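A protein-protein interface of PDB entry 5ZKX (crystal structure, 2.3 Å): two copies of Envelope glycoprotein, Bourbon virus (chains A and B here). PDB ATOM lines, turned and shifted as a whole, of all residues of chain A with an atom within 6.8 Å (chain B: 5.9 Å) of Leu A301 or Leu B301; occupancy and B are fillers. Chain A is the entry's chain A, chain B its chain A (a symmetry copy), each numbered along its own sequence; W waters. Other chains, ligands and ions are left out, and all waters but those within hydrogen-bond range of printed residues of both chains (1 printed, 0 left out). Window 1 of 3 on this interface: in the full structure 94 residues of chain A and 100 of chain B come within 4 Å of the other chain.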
ATOM      1  N   VAL A 295     -24.954  15.475 -24.410  1.00  0.00           N
ATOM      2  CA  VAL A 295     -25.941  16.344 -23.777  1.00  0.00           C
ATOM      3  C   VAL A 295     -25.563  16.599 -22.322  1.00  0.00           C
ATOM      4  O   VAL A 295     -25.646  17.732 -21.832  1.00  0.00           O
ATOM      5  CB  VAL A 295     -27.350  15.732 -23.904  1.00  0.00           C
ATOM      6  CG1 VAL A 295     -28.365  16.555 -23.131  1.00  0.00           C
ATOM      7  CG2 VAL A 295     -27.751  15.622 -25.371  1.00  0.00           C
ATOM      8  N   TYR A 296     -25.129  15.552 -21.616  1.00  0.00           N
ATOM      9  CA  TYR A 296     -24.707  15.700 -20.226  1.00  0.00           C
ATOM     10  C   TYR A 296     -23.529  16.661 -20.100  1.00  0.00           C
ATOM     11  O   TYR A 296     -23.476  17.472 -19.170  1.00  0.00           O
ATOM     12  CB  TYR A 296     -24.350  14.328 -19.653  1.00  0.00           C
ATOM     13  CG  TYR A 296     -24.028  14.311 -18.175  1.00  0.00           C
ATOM     14  CD1 TYR A 296     -22.714  14.376 -17.729  1.00  0.00           C
ATOM     15  CD2 TYR A 296     -25.037  14.208 -17.226  1.00  0.00           C
ATOM     16  CE1 TYR A 296     -22.415  14.351 -16.379  1.00  0.00           C
ATOM     17  CE2 TYR A 296     -24.746  14.179 -15.873  1.00  0.00           C
ATOM     18  CZ  TYR A 296     -23.434  14.253 -15.457  1.00  0.00           C
ATOM     19  OH  TYR A 296     -23.139  14.231 -14.114  1.00  0.00           O
ATOM     20  N   GLU A 297     -22.573  16.579 -21.025  1.00  0.00           N
ATOM     21  CA  GLU A 297     -21.428  17.482 -20.985  1.00  0.00           C
ATOM     22  C   GLU A 297     -21.810  18.891 -21.413  1.00  0.00           C
ATOM     23  O   GLU A 297     -21.225  19.864 -20.927  1.00  0.00           O
ATOM     24  CB  GLU A 297     -20.306  16.950 -21.874  1.00  0.00           C
ATOM     25  CG  GLU A 297     -19.529  15.813 -21.248  1.00  0.00           C
ATOM     26  CD  GLU A 297     -18.751  16.249 -20.024  1.00  0.00           C
ATOM     27  OE1 GLU A 297     -17.736  16.956 -20.192  1.00  0.00           O
ATOM     28  OE2 GLU A 297     -19.156  15.889 -18.898  1.00  0.00           O
ATOM     29  N   THR A 298     -22.775  19.020 -22.323  1.00  0.00           N
ATOM     30  CA  THR A 298     -23.220  20.346 -22.732  1.00  0.00           C
ATOM     31  C   THR A 298     -23.975  21.043 -21.607  1.00  0.00           C
ATOM     32  O   THR A 298     -23.840  22.258 -21.422  1.00  0.00           O
ATOM     33  CB  THR A 298     -24.076  20.237 -23.993  1.00  0.00           C
ATOM     34  OG1 THR A 298     -23.239  19.863 -25.094  1.00  0.00           O
ATOM     35  CG2 THR A 298     -24.753  21.566 -24.311  1.00  0.00           C
ATOM     36  N   GLU A 299     -24.762  20.293 -20.831  1.00  0.00           N
ATOM     37  CA  GLU A 299     -25.415  20.890 -19.673  1.00  0.00           C
ATOM     38  C   GLU A 299     -24.395  21.296 -18.621  1.00  0.00           C
ATOM     39  O   GLU A 299     -24.501  22.376 -18.031  1.00  0.00           O
ATOM     40  CB  GLU A 299     -26.440  19.924 -19.079  1.00  0.00           C
ATOM     41  CG  GLU A 299     -27.681  19.717 -19.936  1.00  0.00           C
ATOM     42  CD  GLU A 299     -28.683  20.854 -19.827  1.00  0.00           C
ATOM     43  OE1 GLU A 299     -29.880  20.569 -19.625  1.00  0.00           O
ATOM     44  OE2 GLU A 299     -28.283  22.030 -19.959  1.00  0.00           O
ATOM     45  N   SER A 300     -23.400  20.440 -18.374  1.00  0.00           N
ATOM     46  CA  SER A 300     -22.322  20.787 -17.456  1.00  0.00           C
ATOM     47  C   SER A 300     -21.576  22.024 -17.932  1.00  0.00           C
ATOM     48  O   SER A 300     -21.210  22.888 -17.128  1.00  0.00           O
ATOM     49  CB  SER A 300     -21.362  19.608 -17.315  1.00  0.00           C
ATOM     50  OG  SER A 300     -20.380  19.863 -16.329  1.00  0.00           O
ATOM     51  N   LEU A 301     -21.336  22.118 -19.241  1.00  0.00           N
ATOM     52  CA  LEU A 301     -20.689  23.299 -19.799  1.00  0.00           C
ATOM     53  C   LEU A 301     -21.547  24.541 -19.593  1.00  0.00           C
ATOM     54  O   LEU A 301     -21.028  25.611 -19.254  1.00  0.00           O
ATOM     55  CB  LEU A 301     -20.399  23.064 -21.284  1.00  0.00           C
ATOM     56  CG  LEU A 301     -19.670  24.105 -22.139  1.00  0.00           C
ATOM     57  CD1 LEU A 301     -20.656  25.064 -22.787  1.00  0.00           C
ATOM     58  CD2 LEU A 301     -18.623  24.860 -21.332  1.00  0.00           C
ATOM     59  N   ARG A 302     -22.862  24.417 -19.779  1.00  0.00           N
ATOM     60  CA  ARG A 302     -23.740  25.572 -19.615  1.00  0.00           C
ATOM     61  C   ARG A 302     -23.749  26.058 -18.171  1.00  0.00           C
ATOM     62  O   ARG A 302     -23.844  27.264 -17.915  1.00  0.00           O
ATOM     63  CB  ARG A 302     -25.155  25.228 -20.079  1.00  0.00           C
ATOM     64  CG  ARG A 302     -25.297  25.140 -21.592  1.00  0.00           C
ATOM     65  CD  ARG A 302     -26.461  24.255 -21.997  1.00  0.00           C
ATOM     66  NE  ARG A 302     -27.755  24.870 -21.726  1.00  0.00           N
ATOM     67  CZ  ARG A 302     -28.313  25.806 -22.489  1.00  0.00           C
ATOM     68  NH1 ARG A 302     -27.682  26.243 -23.570  1.00  0.00           N
ATOM     69  NH2 ARG A 302     -29.500  26.308 -22.170  1.00  0.00           N
ATOM     70  N   LEU A 303     -23.650  25.133 -17.216  1.00  0.00           N
ATOM     71  CA  LEU A 303     -23.551  25.513 -15.810  1.00  0.00           C
ATOM     72  C   LEU A 303     -22.307  26.355 -15.561  1.00  0.00           C
ATOM     73  O   LEU A 303     -22.365  27.382 -14.876  1.00  0.00           O
ATOM     74  CB  LEU A 303     -23.527  24.264 -14.931  1.00  0.00           C
ATOM     75  CG  LEU A 303     -24.846  23.794 -14.319  1.00  0.00           C
ATOM     76  CD1 LEU A 303     -24.572  22.783 -13.215  1.00  0.00           C
ATOM     77  CD2 LEU A 303     -25.641  24.971 -13.784  1.00  0.00           C
ATOM     78  N   SER A 304     -21.165  25.925 -16.104  1.00  0.00           N
ATOM     79  CA  SER A 304     -19.933  26.687 -15.936  1.00  0.00           C
ATOM     80  C   SER A 304     -20.054  28.076 -16.551  1.00  0.00           C
ATOM     81  O   SER A 304     -19.626  29.068 -15.950  1.00  0.00           O
ATOM     82  CB  SER A 304     -18.763  25.929 -16.557  1.00  0.00           C
ATOM     83  OG  SER A 304     -18.591  24.672 -15.931  1.00  0.00           O
ATOM     84  N   LEU A 305     -20.640  28.165 -17.745  1.00  0.00           N
ATOM     85  CA  LEU A 305     -20.787  29.457 -18.407  1.00  0.00           C
ATOM     86  C   LEU A 305     -21.730  30.371 -17.637  1.00  0.00           C
ATOM     87  O   LEU A 305     -21.471  31.575 -17.514  1.00  0.00           O
ATOM     88  CB  LEU A 305     -21.287  29.259 -19.834  1.00  0.00           C
ATOM     89  CG  LEU A 305     -20.254  28.732 -20.818  1.00  0.00           C
ATOM     90  CD1 LEU A 305     -20.882  28.619 -22.186  1.00  0.00           C
ATOM     91  CD2 LEU A 305     -19.041  29.646 -20.850  1.00  0.00           C
ATOM     92  N   ALA A 306     -22.834  29.825 -17.127  1.00  0.00           N
ATOM     93  CA  ALA A 306     -23.745  30.634 -16.329  1.00  0.00           C
ATOM     94  C   ALA A 306     -23.067  31.135 -15.059  1.00  0.00           C
ATOM     95  O   ALA A 306     -23.307  32.266 -14.626  1.00  0.00           O
ATOM     96  CB  ALA A 306     -24.998  29.827 -15.991  1.00  0.00           C
ATOM     97  N   LEU A 406      -8.672  28.796 -26.972  1.00  0.00           N
ATOM     98  CA  LEU A 406      -9.978  28.412 -27.481  1.00  0.00           C
ATOM     99  C   LEU A 406      -9.934  26.992 -28.019  1.00  0.00           C
ATOM    100  O   LEU A 406      -9.061  26.678 -28.841  1.00  0.00           O
ATOM    101  CB  LEU A 406     -10.433  29.368 -28.587  1.00  0.00           C
ATOM    102  CG  LEU A 406     -10.687  30.823 -28.196  1.00  0.00           C
ATOM    103  CD1 LEU A 406     -11.022  31.649 -29.424  1.00  0.00           C
ATOM    104  CD2 LEU A 406     -11.798  30.918 -27.164  1.00  0.00           C
ATOM    105  N   PRO A 407     -10.831  26.111 -27.577  1.00  0.00           N
ATOM    106  CA  PRO A 407     -10.895  24.759 -28.154  1.00  0.00           C
ATOM    107  C   PRO A 407     -11.095  24.818 -29.660  1.00  0.00           C
ATOM    108  O   PRO A 407     -12.047  25.423 -30.156  1.00  0.00           O
ATOM    109  CB  PRO A 407     -12.101  24.130 -27.447  1.00  0.00           C
ATOM    110  CG  PRO A 407     -12.229  24.888 -26.170  1.00  0.00           C
ATOM    111  CD  PRO A 407     -11.777  26.288 -26.462  1.00  0.00           C
ATOM    112  N   TYR B 296     -20.708  21.842 -34.527  1.00  0.00           N
ATOM    113  CA  TYR B 296     -21.661  22.925 -34.306  1.00  0.00           C
ATOM    114  C   TYR B 296     -21.654  23.386 -32.852  1.00  0.00           C
ATOM    115  O   TYR B 296     -21.731  24.587 -32.574  1.00  0.00           O
ATOM    116  CB  TYR B 296     -23.059  22.465 -34.722  1.00  0.00           C
ATOM    117  CG  TYR B 296     -24.128  23.535 -34.679  1.00  0.00           C
ATOM    118  CD1 TYR B 296     -24.957  23.672 -33.572  1.00  0.00           C
ATOM    119  CD2 TYR B 296     -24.324  24.393 -35.753  1.00  0.00           C
ATOM    120  CE1 TYR B 296     -25.943  24.642 -33.533  1.00  0.00           C
ATOM    121  CE2 TYR B 296     -25.309  25.364 -35.723  1.00  0.00           C
ATOM    122  CZ  TYR B 296     -26.114  25.485 -34.610  1.00  0.00           C
ATOM    123  OH  TYR B 296     -27.090  26.452 -34.571  1.00  0.00           O
ATOM    124  N   GLU B 297     -21.569  22.444 -31.913  1.00  0.00           N
ATOM    125  CA  GLU B 297     -21.532  22.811 -30.502  1.00  0.00           C
ATOM    126  C   GLU B 297     -20.190  23.409 -30.113  1.00  0.00           C
ATOM    127  O   GLU B 297     -20.128  24.266 -29.227  1.00  0.00           O
ATOM    128  CB  GLU B 297     -21.834  21.591 -29.633  1.00  0.00           C
ATOM    129  CG  GLU B 297     -23.304  21.237 -29.581  1.00  0.00           C
ATOM    130  CD  GLU B 297     -24.132  22.301 -28.891  1.00  0.00           C
ATOM    131  OE1 GLU B 297     -24.033  22.412 -27.651  1.00  0.00           O
ATOM    132  OE2 GLU B 297     -24.875  23.026 -29.586  1.00  0.00           O
ATOM    133  N   THR B 298     -19.107  22.966 -30.753  1.00  0.00           N
ATOM    134  CA  THR B 298     -17.800  23.541 -30.462  1.00  0.00           C
ATOM    135  C   THR B 298     -17.704  24.974 -30.970  1.00  0.00           C
ATOM    136  O   THR B 298     -17.098  25.830 -30.317  1.00  0.00           O
ATOM    137  CB  THR B 298     -16.704  22.662 -31.062  1.00  0.00           C
ATOM    138  OG1 THR B 298     -16.644  21.429 -30.335  1.00  0.00           O
ATOM    139  CG2 THR B 298     -15.346  23.351 -30.984  1.00  0.00           C
ATOM    140  N   GLU B 299     -18.309  25.262 -32.125  1.00  0.00           N
ATOM    141  CA  GLU B 299     -18.343  26.642 -32.597  1.00  0.00           C
ATOM    142  C   GLU B 299     -19.194  27.508 -31.683  1.00  0.00           C
ATOM    143  O   GLU B 299     -18.815  28.641 -31.364  1.00  0.00           O
ATOM    144  CB  GLU B 299     -18.867  26.704 -34.032  1.00  0.00           C
ATOM    145  CG  GLU B 299     -17.909  26.149 -35.076  1.00  0.00           C
ATOM    146  CD  GLU B 299     -16.791  27.112 -35.438  1.00  0.00           C
ATOM    147  OE1 GLU B 299     -16.557  27.318 -36.645  1.00  0.00           O
ATOM    148  OE2 GLU B 299     -16.135  27.650 -34.522  1.00  0.00           O
ATOM    149  N   SER B 300     -20.348  26.992 -31.251  1.00  0.00           N
ATOM    150  CA  SER B 300     -21.180  27.710 -30.293  1.00  0.00           C
ATOM    151  C   SER B 300     -20.428  27.955 -28.993  1.00  0.00           C
ATOM    152  O   SER B 300     -20.534  29.033 -28.398  1.00  0.00           O
ATOM    153  CB  SER B 300     -22.460  26.922 -30.026  1.00  0.00           C
ATOM    154  OG  SER B 300     -23.350  27.654 -29.204  1.00  0.00           O
ATOM    155  N   LEU B 301     -19.669  26.959 -28.538  1.00  0.00           N
ATOM    156  CA  LEU B 301     -18.858  27.126 -27.338  1.00  0.00           C
ATOM    157  C   LEU B 301     -17.797  28.201 -27.541  1.00  0.00           C
ATOM    158  O   LEU B 301     -17.552  29.016 -26.643  1.00  0.00           O
ATOM    159  CB  LEU B 301     -18.224  25.784 -26.964  1.00  0.00           C
ATOM    160  CG  LEU B 301     -17.357  25.621 -25.711  1.00  0.00           C
ATOM    161  CD1 LEU B 301     -15.893  25.889 -26.024  1.00  0.00           C
ATOM    162  CD2 LEU B 301     -17.843  26.507 -24.573  1.00  0.00           C
ATOM    163  N   ARG B 302     -17.166  28.229 -28.716  1.00  0.00           N
ATOM    164  CA  ARG B 302     -16.127  29.221 -28.969  1.00  0.00           C
ATOM    165  C   ARG B 302     -16.701  30.632 -28.975  1.00  0.00           C
ATOM    166  O   ARG B 302     -16.041  31.581 -28.537  1.00  0.00           O
ATOM    167  CB  ARG B 302     -15.420  28.919 -30.291  1.00  0.00           C
ATOM    168  CG  ARG B 302     -14.479  27.724 -30.220  1.00  0.00           C
ATOM    169  CD  ARG B 302     -14.271  27.091 -31.583  1.00  0.00           C
ATOM    170  NE  ARG B 302     -13.457  27.917 -32.467  1.00  0.00           N
ATOM    171  CZ  ARG B 302     -12.131  28.002 -32.400  1.00  0.00           C
ATOM    172  NH1 ARG B 302     -11.468  27.316 -31.479  1.00  0.00           N
ATOM    173  NH2 ARG B 302     -11.466  28.776 -33.250  1.00  0.00           N
ATOM    174  N   LEU B 303     -17.931  30.788 -29.468  1.00  0.00           N
ATOM    175  CA  LEU B 303     -18.599  32.085 -29.423  1.00  0.00           C
ATOM    176  C   LEU B 303     -18.774  32.557 -27.986  1.00  0.00           C
ATOM    177  O   LEU B 303     -18.510  33.720 -27.666  1.00  0.00           O
ATOM    178  CB  LEU B 303     -19.956  31.998 -30.119  1.00  0.00           C
ATOM    179  CG  LEU B 303     -20.039  32.431 -31.582  1.00  0.00           C
ATOM    180  CD1 LEU B 303     -21.494  32.616 -31.985  1.00  0.00           C
ATOM    181  CD2 LEU B 303     -19.251  33.709 -31.811  1.00  0.00           C
ATOM    182  N   SER B 304     -19.233  31.663 -27.106  1.00  0.00           N
ATOM    183  CA  SER B 304     -19.405  32.025 -25.703  1.00  0.00           C
ATOM    184  C   SER B 304     -18.077  32.419 -25.068  1.00  0.00           C
ATOM    185  O   SER B 304     -18.004  33.405 -24.327  1.00  0.00           O
ATOM    186  CB  SER B 304     -20.039  30.866 -24.940  1.00  0.00           C
ATOM    187  OG  SER B 304     -21.313  30.552 -25.471  1.00  0.00           O
ATOM    188  N   LEU B 305     -17.017  31.661 -25.352  1.00  0.00           N
ATOM    189  CA  LEU B 305     -15.711  31.965 -24.777  1.00  0.00           C
ATOM    190  C   LEU B 305     -15.171  33.291 -25.293  1.00  0.00           C
ATOM    191  O   LEU B 305     -14.591  34.070 -24.528  1.00  0.00           O
ATOM    192  CB  LEU B 305     -14.732  30.837 -25.083  1.00  0.00           C
ATOM    193  CG  LEU B 305     -14.931  29.564 -24.275  1.00  0.00           C
ATOM    194  CD1 LEU B 305     -13.875  28.558 -24.663  1.00  0.00           C
ATOM    195  CD2 LEU B 305     -14.873  29.868 -22.787  1.00  0.00           C
ATOM    196  N   ALA B 306     -15.337  33.558 -26.589  1.00  0.00           N
ATOM    197  CA  ALA B 306     -14.897  34.836 -27.131  1.00  0.00           C
ATOM    198  C   ALA B 306     -15.666  35.994 -26.504  1.00  0.00           C
ATOM    199  O   ALA B 306     -15.096  37.061 -26.255  1.00  0.00           O
ATOM    200  CB  ALA B 306     -15.056  34.840 -28.650  1.00  0.00           C
ATOM    201  N   TRP B 405     -17.367  25.368 -11.287  1.00  0.00           N
ATOM    202  CA  TRP B 405     -17.766  24.054 -11.772  1.00  0.00           C
ATOM    203  C   TRP B 405     -17.106  23.776 -13.117  1.00  0.00           C
ATOM    204  O   TRP B 405     -17.293  24.533 -14.075  1.00  0.00           O
ATOM    205  CB  TRP B 405     -19.285  23.984 -11.904  1.00  0.00           C
ATOM    206  CG  TRP B 405     -19.755  22.787 -12.665  1.00  0.00           C
ATOM    207  CD1 TRP B 405     -20.328  22.773 -13.904  1.00  0.00           C
ATOM    208  CD2 TRP B 405     -19.686  21.424 -12.238  1.00  0.00           C
ATOM    209  NE1 TRP B 405     -20.622  21.484 -14.273  1.00  0.00           N
ATOM    210  CE2 TRP B 405     -20.237  20.636 -13.267  1.00  0.00           C
ATOM    211  CE3 TRP B 405     -19.212  20.791 -11.085  1.00  0.00           C
ATOM    212  CZ2 TRP B 405     -20.328  19.249 -13.177  1.00  0.00           C
ATOM    213  CZ3 TRP B 405     -19.302  19.413 -10.997  1.00  0.00           C
ATOM    214  CH2 TRP B 405     -19.855  18.658 -12.037  1.00  0.00           C
ATOM    215  N   PRO B 407     -16.714  20.994 -16.230  1.00  0.00           N
ATOM    216  CA  PRO B 407     -17.198  19.738 -16.824  1.00  0.00           C
ATOM    217  C   PRO B 407     -16.140  18.650 -16.738  1.00  0.00           C
ATOM    218  O   PRO B 407     -15.014  18.814 -17.208  1.00  0.00           O
ATOM    219  CB  PRO B 407     -17.494  20.127 -18.277  1.00  0.00           C
ATOM    220  CG  PRO B 407     -17.736  21.597 -18.235  1.00  0.00           C
ATOM    221  CD  PRO B 407     -16.860  22.138 -17.145  1.00  0.00           C
HETATM  222  O   HOH W   1     -21.668  21.288 -26.302  1.00  0.00           O
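The side-chain hydroxyl of Ser A300 is in hydrogen-bond range of the indole nitrogen of Trp B405 (2.6 Å).
The side-chain hydroxyl of Ser A304 sits close to the backbone carbonyl oxygen of Trp B405.
O of Pro A407 sits close to NH1 of Arg B302, 2.4 Å away.
O of Ser A300 is in hydrogen-bond range of OG of Ser A304 (3.4 Å).
The side-chain carboxylate of Glu B299 is in salt-bridge range of the guanidinium group of Arg B302 (3.4 Å).
OG of Ser B304 is in hydrogen-bond range of O of Ser B300.
Glu A297 touches Pro B407 (OE1 to CB, 3.7 Å).
Glu B297 touches Thr A298 (OE1 to CG2, 3.5 Å).
OG of Ser A300 touches CA of Pro B407, at 3.2 Å.
Leu A301 touches Pro B407 (CA to CG, 3.8 Å).
OG of Ser A304 touches CD of Pro B407 (3.3 Å).
CD1 of Leu A305 touches CB of Ser B304, 3.7 Å away.
NH1 of Arg B302 touches O of Leu A406 (3.6 Å).
Pro A407 touches Thr B298.
Pro A407 touches Leu B301.
Pro A407 touches Leu B305 (CD to CD1, 3.6 Å).
Of chain A, only Leu A301 and Pro A407 come within 4 Å of Leu B301.
Of the printed residues of chain A, Arg B302 touches Leu A406 and Pro A407.
Of the printed residues of chain A, Thr B298 touches Pro A407 (3.98 Å).
The nearest residue of chain A that does not touch Leu B301 is Leu A305 (4.4 Å).
The nearest printed residue of chain B that does not touch Leu A406 is Ala B306 (4.5 Å).
Hydrophobic or aromatic side chains of chain B that line the printed part of chain A: Leu B301, Leu B305, Trp B405 and Pro B407.
Of the 14 printed residues of chain A, 9 touch a printed residue of chain B.
Among the printed residues, 16 pairs touch across the chains.
Glu A297 touches Pro B407, but with the chains exchanged Pro A407 does not touch Glu B297 (8.2 Å).
Leu B301 touches its own counterpart, Leu A301.
Ser A304 touches Pro B407, but with the chains exchanged Pro A407 does not touch Ser B304 (8.9 Å).
Pro A407 touches Leu B305, but with the chains exchanged Leu A305 does not touch Pro B407 (7.1 Å).
12 positions are printed for both chains.
Of the 16 pairs that touch across the chains among the printed residues, 3 have their exchanged pair printed and touching as well.
Water W1 lies within hydrogen-bond range of the side-chain hydroxyl (OG1) of Thr A298 (2.4 Å) and the side-chain carboxylate (OE1) of Glu B297 (2.9 Å).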
